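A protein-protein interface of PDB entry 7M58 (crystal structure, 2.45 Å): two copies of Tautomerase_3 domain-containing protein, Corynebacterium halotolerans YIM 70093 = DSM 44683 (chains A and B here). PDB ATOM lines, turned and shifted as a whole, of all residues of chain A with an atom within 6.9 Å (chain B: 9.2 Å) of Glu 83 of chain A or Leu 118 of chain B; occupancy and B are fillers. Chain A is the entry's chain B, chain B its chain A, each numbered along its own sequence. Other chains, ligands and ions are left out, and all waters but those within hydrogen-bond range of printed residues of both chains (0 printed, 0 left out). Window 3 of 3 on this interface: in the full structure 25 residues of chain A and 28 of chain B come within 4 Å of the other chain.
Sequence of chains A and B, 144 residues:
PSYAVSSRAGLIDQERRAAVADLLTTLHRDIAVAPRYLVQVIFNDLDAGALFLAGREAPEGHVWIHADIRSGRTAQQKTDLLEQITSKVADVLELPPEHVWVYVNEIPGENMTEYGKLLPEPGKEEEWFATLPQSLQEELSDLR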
ATOM      1  N   LYS A  78      24.540  -1.404  12.455  1.00  0.00           N
ATOM      2  CA  LYS A  78      24.258  -2.796  12.748  1.00  0.00           C
ATOM      3  C   LYS A  78      25.271  -3.369  13.730  1.00  0.00           C
ATOM      4  O   LYS A  78      24.901  -3.958  14.751  1.00  0.00           O
ATOM      5  CB  LYS A  78      24.232  -3.590  11.445  1.00  0.00           C
ATOM      6  CG  LYS A  78      22.926  -3.474  10.675  1.00  0.00           C
ATOM      7  CD  LYS A  78      22.916  -4.410   9.488  1.00  0.00           C
ATOM      8  CE  LYS A  78      23.199  -3.595   8.254  1.00  0.00           C
ATOM      9  NZ  LYS A  78      23.589  -4.406   7.079  1.00  0.00           N
ATOM     10  N   THR A  79      26.560  -3.199  13.447  1.00  0.00           N
ATOM     11  CA  THR A  79      27.557  -3.803  14.322  1.00  0.00           C
ATOM     12  C   THR A  79      27.545  -3.149  15.696  1.00  0.00           C
ATOM     13  O   THR A  79      27.753  -3.822  16.714  1.00  0.00           O
ATOM     14  CB  THR A  79      28.942  -3.709  13.684  1.00  0.00           C
ATOM     15  OG1 THR A  79      29.195  -2.349  13.326  1.00  0.00           O
ATOM     16  CG2 THR A  79      29.017  -4.586  12.418  1.00  0.00           C
ATOM     17  N   ASP A  80      27.273  -1.853  15.753  1.00  0.00           N
ATOM     18  CA  ASP A  80      27.161  -1.218  17.055  1.00  0.00           C
ATOM     19  C   ASP A  80      25.955  -1.762  17.820  1.00  0.00           C
ATOM     20  O   ASP A  80      26.057  -2.088  19.012  1.00  0.00           O
ATOM     21  CB  ASP A  80      27.067   0.296  16.885  1.00  0.00           C
ATOM     22  CG  ASP A  80      28.020   1.033  17.802  1.00  0.00           C
ATOM     23  OD1 ASP A  80      28.190   0.600  18.973  1.00  0.00           O
ATOM     24  OD2 ASP A  80      28.649   2.013  17.331  1.00  0.00           O
ATOM     25  N   LEU A  81      24.819  -1.922  17.138  1.00  0.00           N
ATOM     26  CA  LEU A  81      23.642  -2.494  17.783  1.00  0.00           C
ATOM     27  C   LEU A  81      23.912  -3.904  18.297  1.00  0.00           C
ATOM     28  O   LEU A  81      23.495  -4.263  19.402  1.00  0.00           O
ATOM     29  CB  LEU A  81      22.469  -2.496  16.804  1.00  0.00           C
ATOM     30  CG  LEU A  81      21.079  -2.918  17.276  1.00  0.00           C
ATOM     31  CD1 LEU A  81      20.435  -1.875  18.201  1.00  0.00           C
ATOM     32  CD2 LEU A  81      20.205  -3.188  16.082  1.00  0.00           C
ATOM     33  N   LEU A  82      24.627  -4.709  17.516  1.00  0.00           N
ATOM     34  CA  LEU A  82      24.884  -6.096  17.886  1.00  0.00           C
ATOM     35  C   LEU A  82      25.781  -6.179  19.111  1.00  0.00           C
ATOM     36  O   LEU A  82      25.488  -6.913  20.063  1.00  0.00           O
ATOM     37  CB  LEU A  82      25.514  -6.812  16.695  1.00  0.00           C
ATOM     38  CG  LEU A  82      24.457  -7.269  15.697  1.00  0.00           C
ATOM     39  CD1 LEU A  82      25.016  -7.236  14.307  1.00  0.00           C
ATOM     40  CD2 LEU A  82      24.057  -8.661  16.063  1.00  0.00           C
ATOM     41  N   GLU A  83      26.890  -5.444  19.094  1.00  0.00           N
ATOM     42  CA  GLU A  83      27.823  -5.480  20.212  1.00  0.00           C
ATOM     43  C   GLU A  83      27.198  -4.916  21.481  1.00  0.00           C
ATOM     44  O   GLU A  83      27.406  -5.465  22.573  1.00  0.00           O
ATOM     45  CB  GLU A  83      29.085  -4.725  19.838  1.00  0.00           C
ATOM     46  CG  GLU A  83      29.754  -5.362  18.650  1.00  0.00           C
ATOM     47  CD  GLU A  83      31.086  -4.732  18.322  1.00  0.00           C
ATOM     48  OE1 GLU A  83      32.066  -5.490  18.127  1.00  0.00           O
ATOM     49  OE2 GLU A  83      31.141  -3.479  18.243  1.00  0.00           O
ATOM     50  N   GLN A  84      26.400  -3.847  21.359  1.00  0.00           N
ATOM     51  CA  GLN A  84      25.808  -3.238  22.552  1.00  0.00           C
ATOM     52  C   GLN A  84      24.665  -4.075  23.126  1.00  0.00           C
ATOM     53  O   GLN A  84      24.509  -4.150  24.352  1.00  0.00           O
ATOM     54  CB  GLN A  84      25.322  -1.840  22.211  1.00  0.00           C
ATOM     55  CG  GLN A  84      26.449  -0.829  22.029  1.00  0.00           C
ATOM     56  CD  GLN A  84      25.947   0.576  22.182  1.00  0.00           C
ATOM     57  OE1 GLN A  84      25.298   0.910  23.171  1.00  0.00           O
ATOM     58  NE2 GLN A  84      26.201   1.405  21.173  1.00  0.00           N
ATOM     59  N   ILE A  85      23.882  -4.743  22.279  1.00  0.00           N
ATOM     60  CA  ILE A  85      22.852  -5.633  22.794  1.00  0.00           C
ATOM     61  C   ILE A  85      23.488  -6.794  23.537  1.00  0.00           C
ATOM     62  O   ILE A  85      23.101  -7.109  24.654  1.00  0.00           O
ATOM     63  CB  ILE A  85      21.960  -6.141  21.653  1.00  0.00           C
ATOM     64  CG1 ILE A  85      21.015  -5.056  21.161  1.00  0.00           C
ATOM     65  CG2 ILE A  85      21.185  -7.358  22.090  1.00  0.00           C
ATOM     66  CD1 ILE A  85      20.331  -5.439  19.863  1.00  0.00           C
ATOM     67  N   THR A  86      24.487  -7.432  22.919  1.00  0.00           N
ATOM     68  CA  THR A  86      25.217  -8.534  23.542  1.00  0.00           C
ATOM     69  C   THR A  86      25.858  -8.124  24.863  1.00  0.00           C
ATOM     70  O   THR A  86      25.852  -8.900  25.818  1.00  0.00           O
ATOM     71  CB  THR A  86      26.288  -9.069  22.585  1.00  0.00           C
ATOM     72  OG1 THR A  86      25.728  -9.355  21.291  1.00  0.00           O
ATOM     73  CG2 THR A  86      26.958 -10.322  23.144  1.00  0.00           C
ATOM     74  N   SER A  87      26.435  -6.922  24.931  1.00  0.00           N
ATOM     75  CA  SER A  87      27.143  -6.492  26.139  1.00  0.00           C
ATOM     76  C   SER A  87      26.187  -6.046  27.239  1.00  0.00           C
ATOM     77  O   SER A  87      26.318  -6.468  28.393  1.00  0.00           O
ATOM     78  CB  SER A  87      28.116  -5.360  25.817  1.00  0.00           C
ATOM     79  OG  SER A  87      29.294  -5.903  25.265  1.00  0.00           O
ATOM     80  N   LYS A  88      25.241  -5.166  26.914  1.00  0.00           N
ATOM     81  CA  LYS A  88      24.400  -4.604  27.961  1.00  0.00           C
ATOM     82  C   LYS A  88      23.289  -5.555  28.411  1.00  0.00           C
ATOM     83  O   LYS A  88      22.910  -5.536  29.592  1.00  0.00           O
ATOM     84  CB  LYS A  88      23.859  -3.261  27.505  1.00  0.00           C
ATOM     85  CG  LYS A  88      24.990  -2.333  27.107  1.00  0.00           C
ATOM     86  CD  LYS A  88      24.518  -0.915  26.809  1.00  0.00           C
ATOM     87  CE  LYS A  88      25.623  -0.130  26.098  1.00  0.00           C
ATOM     88  NZ  LYS A  88      25.267   1.293  25.778  1.00  0.00           N
ATOM     89  N   VAL A  89      22.768  -6.404  27.522  1.00  0.00           N
ATOM     90  CA  VAL A  89      21.801  -7.393  27.986  1.00  0.00           C
ATOM     91  C   VAL A  89      22.491  -8.423  28.867  1.00  0.00           C
ATOM     92  O   VAL A  89      21.952  -8.841  29.900  1.00  0.00           O
ATOM     93  CB  VAL A  89      21.070  -8.066  26.813  1.00  0.00           C
ATOM     94  CG1 VAL A  89      20.368  -9.319  27.296  1.00  0.00           C
ATOM     95  CG2 VAL A  89      20.054  -7.112  26.226  1.00  0.00           C
ATOM     96  N   VAL A 102      23.182 -12.920  19.584  1.00  0.00           N
ATOM     97  CA  VAL A 102      22.285 -11.986  18.905  1.00  0.00           C
ATOM     98  C   VAL A 102      22.370 -12.174  17.398  1.00  0.00           C
ATOM     99  O   VAL A 102      23.466 -12.160  16.827  1.00  0.00           O
ATOM    100  CB  VAL A 102      22.608 -10.522  19.255  1.00  0.00           C
ATOM    101  CG1 VAL A 102      21.486  -9.620  18.772  1.00  0.00           C
ATOM    102  CG2 VAL A 102      22.841 -10.353  20.753  1.00  0.00           C
ATOM    103  N   LEU B  38      29.507 -23.800  17.375  1.00  0.00           N
ATOM    104  CA  LEU B  38      28.694 -22.696  16.894  1.00  0.00           C
ATOM    105  C   LEU B  38      27.210 -23.030  16.853  1.00  0.00           C
ATOM    106  O   LEU B  38      26.390 -22.123  16.683  1.00  0.00           O
ATOM    107  CB  LEU B  38      29.146 -22.273  15.493  1.00  0.00           C
ATOM    108  CG  LEU B  38      30.486 -21.534  15.352  1.00  0.00           C
ATOM    109  CD1 LEU B  38      30.606 -20.893  13.969  1.00  0.00           C
ATOM    110  CD2 LEU B  38      30.682 -20.512  16.440  1.00  0.00           C
ATOM    111  N   ARG B  70      24.778 -18.636   8.123  1.00  0.00           N
ATOM    112  CA  ARG B  70      25.487 -17.538   7.482  1.00  0.00           C
ATOM    113  C   ARG B  70      25.342 -17.586   5.966  1.00  0.00           C
ATOM    114  O   ARG B  70      25.343 -18.659   5.352  1.00  0.00           O
ATOM    115  CB  ARG B  70      26.961 -17.590   7.862  1.00  0.00           C
ATOM    116  CG  ARG B  70      27.245 -16.890   9.140  1.00  0.00           C
ATOM    117  CD  ARG B  70      28.628 -17.166   9.663  1.00  0.00           C
ATOM    118  NE  ARG B  70      28.846 -18.596   9.857  1.00  0.00           N
ATOM    119  CZ  ARG B  70      30.042 -19.157   9.997  1.00  0.00           C
ATOM    120  NH1 ARG B  70      31.133 -18.407   9.980  1.00  0.00           N
ATOM    121  NH2 ARG B  70      30.144 -20.471  10.142  1.00  0.00           N
ATOM    122  N   PRO B 108      24.105 -12.604   6.948  1.00  0.00           N
ATOM    123  CA  PRO B 108      25.554 -12.370   6.990  1.00  0.00           C
ATOM    124  C   PRO B 108      26.137 -12.632   8.373  1.00  0.00           C
ATOM    125  O   PRO B 108      25.476 -12.458   9.399  1.00  0.00           O
ATOM    126  CB  PRO B 108      25.685 -10.893   6.598  1.00  0.00           C
ATOM    127  CG  PRO B 108      24.289 -10.348   6.601  1.00  0.00           C
ATOM    128  CD  PRO B 108      23.385 -11.473   6.356  1.00  0.00           C
ATOM    129  N   GLY B 109      27.388 -13.100   8.383  1.00  0.00           N
ATOM    130  CA  GLY B 109      28.062 -13.399   9.638  1.00  0.00           C
ATOM    131  C   GLY B 109      28.200 -12.191  10.547  1.00  0.00           C
ATOM    132  O   GLY B 109      28.053 -12.303  11.763  1.00  0.00           O
ATOM    133  N   GLU B 110      28.513 -11.024   9.978  1.00  0.00           N
ATOM    134  CA  GLU B 110      28.596  -9.816  10.796  1.00  0.00           C
ATOM    135  C   GLU B 110      27.279  -9.450  11.458  1.00  0.00           C
ATOM    136  O   GLU B 110      27.279  -8.593  12.351  1.00  0.00           O
ATOM    137  CB  GLU B 110      29.102  -8.615   9.986  1.00  0.00           C
ATOM    138  CG  GLU B 110      28.246  -8.200   8.806  1.00  0.00           C
ATOM    139  CD  GLU B 110      28.682  -8.838   7.476  1.00  0.00           C
ATOM    140  OE1 GLU B 110      28.479  -8.184   6.418  1.00  0.00           O
ATOM    141  OE2 GLU B 110      29.221  -9.975   7.479  1.00  0.00           O
ATOM    142  N   ASN B 111      26.169 -10.076  11.062  1.00  0.00           N
ATOM    143  CA  ASN B 111      24.891  -9.880  11.731  1.00  0.00           C
ATOM    144  C   ASN B 111      24.659 -10.901  12.836  1.00  0.00           C
ATOM    145  O   ASN B 111      23.517 -11.134  13.232  1.00  0.00           O
ATOM    146  CB  ASN B 111      23.744  -9.916  10.715  1.00  0.00           C
ATOM    147  CG  ASN B 111      23.781  -8.745   9.732  1.00  0.00           C
ATOM    148  OD1 ASN B 111      24.829  -8.165   9.461  1.00  0.00           O
ATOM    149  ND2 ASN B 111      22.630  -8.413   9.181  1.00  0.00           N
ATOM    150  N   MET B 112      25.715 -11.532  13.331  1.00  0.00           N
ATOM    151  CA  MET B 112      25.585 -12.514  14.392  1.00  0.00           C
ATOM    152  C   MET B 112      26.686 -12.306  15.415  1.00  0.00           C
ATOM    153  O   MET B 112      27.839 -12.068  15.038  1.00  0.00           O
ATOM    154  CB  MET B 112      25.679 -13.940  13.866  1.00  0.00           C
ATOM    155  CG  MET B 112      24.641 -14.273  12.855  1.00  0.00           C
ATOM    156  SD  MET B 112      24.476 -16.041  12.562  1.00  0.00           S
ATOM    157  CE  MET B 112      26.060 -16.513  12.065  1.00  0.00           C
ATOM    158  N   THR B 113      26.329 -12.357  16.695  1.00  0.00           N
ATOM    159  CA  THR B 113      27.295 -12.572  17.763  1.00  0.00           C
ATOM    160  C   THR B 113      27.028 -13.950  18.348  1.00  0.00           C
ATOM    161  O   THR B 113      25.877 -14.351  18.525  1.00  0.00           O
ATOM    162  CB  THR B 113      27.245 -11.515  18.887  1.00  0.00           C
ATOM    163  OG1 THR B 113      25.983 -11.568  19.572  1.00  0.00           O
ATOM    164  CG2 THR B 113      27.490 -10.127  18.356  1.00  0.00           C
ATOM    165  N   GLU B 114      28.105 -14.672  18.609  1.00  0.00           N
ATOM    166  CA  GLU B 114      28.102 -15.909  19.368  1.00  0.00           C
ATOM    167  C   GLU B 114      29.401 -15.910  20.160  1.00  0.00           C
ATOM    168  O   GLU B 114      30.445 -15.494  19.644  1.00  0.00           O
ATOM    169  CB  GLU B 114      28.024 -17.139  18.453  1.00  0.00           C
ATOM    170  CG  GLU B 114      26.726 -17.291  17.681  1.00  0.00           C
ATOM    171  CD  GLU B 114      26.668 -18.611  16.904  1.00  0.00           C
ATOM    172  OE1 GLU B 114      27.533 -19.490  17.165  1.00  0.00           O
ATOM    173  OE2 GLU B 114      25.755 -18.788  16.048  1.00  0.00           O
ATOM    174  N   TYR B 115      29.327 -16.344  21.421  1.00  0.00           N
ATOM    175  CA  TYR B 115      30.464 -16.270  22.343  1.00  0.00           C
ATOM    176  C   TYR B 115      30.995 -14.845  22.480  1.00  0.00           C
ATOM    177  O   TYR B 115      32.196 -14.629  22.637  1.00  0.00           O
ATOM    178  CB  TYR B 115      31.574 -17.236  21.920  1.00  0.00           C
ATOM    179  CG  TYR B 115      31.046 -18.638  21.861  1.00  0.00           C
ATOM    180  CD1 TYR B 115      30.756 -19.339  23.032  1.00  0.00           C
ATOM    181  CD2 TYR B 115      30.807 -19.257  20.652  1.00  0.00           C
ATOM    182  CE1 TYR B 115      30.253 -20.621  22.998  1.00  0.00           C
ATOM    183  CE2 TYR B 115      30.311 -20.545  20.604  1.00  0.00           C
ATOM    184  CZ  TYR B 115      30.036 -21.217  21.782  1.00  0.00           C
ATOM    185  OH  TYR B 115      29.539 -22.486  21.740  1.00  0.00           O
ATOM    186  N   GLY B 116      30.098 -13.867  22.418  1.00  0.00           N
ATOM    187  CA  GLY B 116      30.449 -12.476  22.623  1.00  0.00           C
ATOM    188  C   GLY B 116      31.170 -11.786  21.480  1.00  0.00           C
ATOM    189  O   GLY B 116      31.634 -10.652  21.660  1.00  0.00           O
ATOM    190  N   LYS B 117      31.265 -12.408  20.309  1.00  0.00           N
ATOM    191  CA  LYS B 117      32.071 -11.844  19.235  1.00  0.00           C
ATOM    192  C   LYS B 117      31.321 -11.955  17.918  1.00  0.00           C
ATOM    193  O   LYS B 117      30.624 -12.945  17.683  1.00  0.00           O
ATOM    194  CB  LYS B 117      33.433 -12.552  19.143  1.00  0.00           C
ATOM    195  CG  LYS B 117      34.564 -11.842  19.911  1.00  0.00           C
ATOM    196  CD  LYS B 117      34.653 -12.309  21.366  1.00  0.00           C
ATOM    197  CE  LYS B 117      35.520 -11.382  22.229  1.00  0.00           C
ATOM    198  NZ  LYS B 117      34.964  -9.992  22.336  1.00  0.00           N
ATOM    199  N   LEU B 118      31.452 -10.939  17.065  1.00  0.00           N
ATOM    200  CA  LEU B 118      30.811 -11.015  15.758  1.00  0.00           C
ATOM    201  C   LEU B 118      31.393 -12.190  14.997  1.00  0.00           C
ATOM    202  O   LEU B 118      32.579 -12.496  15.120  1.00  0.00           O
ATOM    203  CB  LEU B 118      31.000  -9.719  14.970  1.00  0.00           C
ATOM    204  CG  LEU B 118      30.164  -8.583  15.557  1.00  0.00           C
ATOM    205  CD1 LEU B 118      30.650  -7.216  15.124  1.00  0.00           C
ATOM    206  CD2 LEU B 118      28.707  -8.776  15.182  1.00  0.00           C
ATOM    207  N   LEU B 119      30.544 -12.892  14.288  1.00  0.00           N
ATOM    208  CA  LEU B 119      30.966 -14.097  13.588  1.00  0.00           C
ATOM    209  C   LEU B 119      31.561 -13.739  12.236  1.00  0.00           C
ATOM    210  O   LEU B 119      31.198 -12.718  11.646  1.00  0.00           O
ATOM    211  CB  LEU B 119      29.792 -15.045  13.379  1.00  0.00           C
ATOM    212  CG  LEU B 119      29.338 -15.838  14.597  1.00  0.00           C
ATOM    213  CD1 LEU B 119      28.485 -17.035  14.196  1.00  0.00           C
ATOM    214  CD2 LEU B 119      30.546 -16.304  15.404  1.00  0.00           C
ATOM    215  N   PRO B 120      32.494 -14.533  11.728  1.00  0.00           N
ATOM    216  CA  PRO B 120      33.070 -14.222  10.422  1.00  0.00           C
ATOM    217  C   PRO B 120      32.318 -14.894   9.294  1.00  0.00           C
ATOM    218  O   PRO B 120      31.422 -15.721   9.511  1.00  0.00           O
ATOM    219  CB  PRO B 120      34.480 -14.796  10.534  1.00  0.00           C
ATOM    220  CG  PRO B 120      34.211 -16.076  11.307  1.00  0.00           C
ATOM    221  CD  PRO B 120      33.120 -15.734  12.313  1.00  0.00           C
ATOM    222  N   GLU B 121      32.744 -14.537   8.082  1.00  0.00           N
ATOM    223  CA  GLU B 121      32.532 -15.342   6.888  1.00  0.00           C
ATOM    224  C   GLU B 121      32.684 -16.847   7.113  1.00  0.00           C
ATOM    225  O   GLU B 121      33.597 -17.292   7.831  1.00  0.00           O
ATOM    226  CB  GLU B 121      33.573 -14.938   5.859  1.00  0.00           C
ATOM    227  CG  GLU B 121      33.637 -15.800   4.660  1.00  0.00           C
ATOM    228  CD  GLU B 121      34.528 -15.267   3.583  1.00  0.00           C
ATOM    229  OE1 GLU B 121      34.584 -14.033   3.452  1.00  0.00           O
ATOM    230  OE2 GLU B 121      35.388 -16.046   3.046  1.00  0.00           O
ATOM    231  N   LYS B 124      36.199 -18.997   7.417  1.00  0.00           N
ATOM    232  CA  LYS B 124      37.209 -18.245   8.145  1.00  0.00           C
ATOM    233  C   LYS B 124      37.167 -18.493   9.653  1.00  0.00           C
ATOM    234  O   LYS B 124      37.490 -17.594  10.437  1.00  0.00           O
ATOM    235  CB  LYS B 124      37.048 -16.762   7.823  1.00  0.00           C
ATOM    236  CG  LYS B 124      37.309 -16.477   6.358  1.00  0.00           C
ATOM    237  CD  LYS B 124      38.782 -16.122   6.110  1.00  0.00           C
ATOM    238  CE  LYS B 124      39.230 -16.580   4.726  1.00  0.00           C
ATOM    239  NZ  LYS B 124      38.172 -16.456   3.656  1.00  0.00           N
ATOM    240  N   GLU B 125      36.729 -19.677  10.084  1.00  0.00           N
ATOM    241  CA  GLU B 125      36.592 -19.924  11.515  1.00  0.00           C
ATOM    242  C   GLU B 125      37.943 -20.030  12.221  1.00  0.00           C
ATOM    243  O   GLU B 125      38.036 -19.667  13.397  1.00  0.00           O
ATOM    244  CB  GLU B 125      35.774 -21.190  11.767  1.00  0.00           C
ATOM    245  CG  GLU B 125      34.298 -21.050  11.449  1.00  0.00           C
ATOM    246  CD  GLU B 125      33.972 -21.335   9.997  1.00  0.00           C
ATOM    247  OE1 GLU B 125      34.872 -21.842   9.295  1.00  0.00           O
ATOM    248  OE2 GLU B 125      32.820 -21.069   9.565  1.00  0.00           O
ATOM    249  N   GLU B 127      40.762 -18.296  11.536  1.00  0.00           N
ATOM    250  CA  GLU B 127      41.144 -16.908  11.760  1.00  0.00           C
ATOM    251  C   GLU B 127      40.357 -16.309  12.925  1.00  0.00           C
ATOM    252  O   GLU B 127      40.934 -15.677  13.812  1.00  0.00           O
ATOM    253  CB  GLU B 127      40.950 -16.103  10.470  1.00  0.00           C
ATOM    254  CG  GLU B 127      42.232 -15.516   9.890  1.00  0.00           C
ATOM    255  CD  GLU B 127      41.972 -14.661   8.661  1.00  0.00           C
ATOM    256  OE1 GLU B 127      42.833 -13.801   8.331  1.00  0.00           O
ATOM    257  OE2 GLU B 127      40.880 -14.800   8.040  1.00  0.00           O
ATOM    258  N   TRP B 128      39.032 -16.486  12.905  1.00  0.00           N
ATOM    259  CA  TRP B 128      38.174 -15.973  13.980  1.00  0.00           C
ATOM    260  C   TRP B 128      38.598 -16.552  15.328  1.00  0.00           C
ATOM    261  O   TRP B 128      38.797 -15.808  16.301  1.00  0.00           O
ATOM    262  CB  TRP B 128      36.707 -16.313  13.646  1.00  0.00           C
ATOM    263  CG  TRP B 128      35.686 -15.960  14.668  1.00  0.00           C
ATOM    264  CD1 TRP B 128      35.043 -14.764  14.806  1.00  0.00           C
ATOM    265  CD2 TRP B 128      35.162 -16.821  15.696  1.00  0.00           C
ATOM    266  NE1 TRP B 128      34.158 -14.818  15.864  1.00  0.00           N
ATOM    267  CE2 TRP B 128      34.215 -16.069  16.430  1.00  0.00           C
ATOM    268  CE3 TRP B 128      35.417 -18.139  16.080  1.00  0.00           C
ATOM    269  CZ2 TRP B 128      33.514 -16.600  17.525  1.00  0.00           C
ATOM    270  CZ3 TRP B 128      34.722 -18.668  17.166  1.00  0.00           C
ATOM    271  CH2 TRP B 128      33.786 -17.895  17.880  1.00  0.00           C
ATOM    272  N   PHE B 129      38.804 -17.871  15.374  1.00  0.00           N
ATOM    273  CA  PHE B 129      39.180 -18.553  16.609  1.00  0.00           C
ATOM    274  C   PHE B 129      40.476 -17.988  17.194  1.00  0.00           C
ATOM    275  O   PHE B 129      40.591 -17.826  18.420  1.00  0.00           O
ATOM    276  CB  PHE B 129      39.309 -20.048  16.316  1.00  0.00           C
ATOM    277  CG  PHE B 129      39.588 -20.891  17.517  1.00  0.00           C
ATOM    278  CD1 PHE B 129      38.557 -21.309  18.345  1.00  0.00           C
ATOM    279  CD2 PHE B 129      40.882 -21.275  17.822  1.00  0.00           C
ATOM    280  CE1 PHE B 129      38.817 -22.090  19.454  1.00  0.00           C
ATOM    281  CE2 PHE B 129      41.141 -22.060  18.934  1.00  0.00           C
ATOM    282  CZ  PHE B 129      40.109 -22.458  19.747  1.00  0.00           C
ATOM    283  N   THR B 131      41.475 -15.051  17.275  1.00  0.00           N
ATOM    284  CA  THR B 131      41.194 -13.761  17.900  1.00  0.00           C
ATOM    285  C   THR B 131      40.573 -13.892  19.288  1.00  0.00           C
ATOM    286  O   THR B 131      40.587 -12.924  20.049  1.00  0.00           O
ATOM    287  CB  THR B 131      40.274 -12.936  16.990  1.00  0.00           C
ATOM    288  OG1 THR B 131      40.813 -12.924  15.662  1.00  0.00           O
ATOM    289  CG2 THR B 131      40.175 -11.492  17.455  1.00  0.00           C
ATOM    290  N   LEU B 132      40.023 -15.049  19.648  1.00  0.00           N
ATOM    291  CA  LEU B 132      39.362 -15.155  20.934  1.00  0.00           C
ATOM    292  C   LEU B 132      40.382 -15.130  22.075  1.00  0.00           C
ATOM    293  O   LEU B 132      41.548 -15.489  21.895  1.00  0.00           O
ATOM    294  CB  LEU B 132      38.494 -16.413  20.992  1.00  0.00           C
ATOM    295  CG  LEU B 132      37.531 -16.564  19.809  1.00  0.00           C
ATOM    296  CD1 LEU B 132      36.623 -17.748  19.961  1.00  0.00           C
ATOM    297  CD2 LEU B 132      36.682 -15.302  19.676  1.00  0.00           C
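OG1 of Thr 113 of chain B sits at hydrogen-bond distance from OG1 of Thr 86 of chain A. The backbone carbonyl oxygen (O) of Val 102 of chain A sits at hydrogen-bond distance from the backbone NH (N) of Thr 113 of chain B (2.9 Å).
The backbone carbonyl oxygen of Met 112 of chain B is in hydrogen-bond range of the backbone NH of Leu 119 of chain B, 2.9 Å away. The backbone carbonyl oxygen (O) of Leu 118 of chain B sits at hydrogen-bond distance from the indole nitrogen (NE1) of Trp 128 of chain B, at 2.9 Å. OG1 of Thr 86 of chain A is in hydrogen-bond range of O of Leu 82 of chain A. The backbone carbonyl oxygen (O) of Glu 83 of chain A sits at hydrogen-bond distance from the side-chain hydroxyl (OG) of Ser 87 of chain A (3.3 Å).
Leu 82 of chain A touches Glu 110 of chain B. Leu 82 of chain A touches Asn 111 of chain B (CD1 to CA, 3.7 Å). Leu 118 of chain B touches Glu 83 of chain A. Val 102 of chain A touches Asn 111 of chain B (O to O, 3.7 Å). Val 102 of chain A touches Met 112 of chain B (O to CA, 3.2 Å).
Of the printed residues of chain A, Met 112 of chain B touches Val 102 (3.2 Å). Of the printed residues of chain A, Thr 113 of chain B touches Thr 86 (2.8 Å) and Val 102 (2.9 Å). Of the printed residues of chain B, Val 102 of chain A touches Asn 111 (3.7 Å), Met 112 (3.2 Å) and Thr 113 (2.9 Å).
Of the 13 printed residues of chain A, 4 touch a printed residue of chain B.
No position is printed for both chains.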
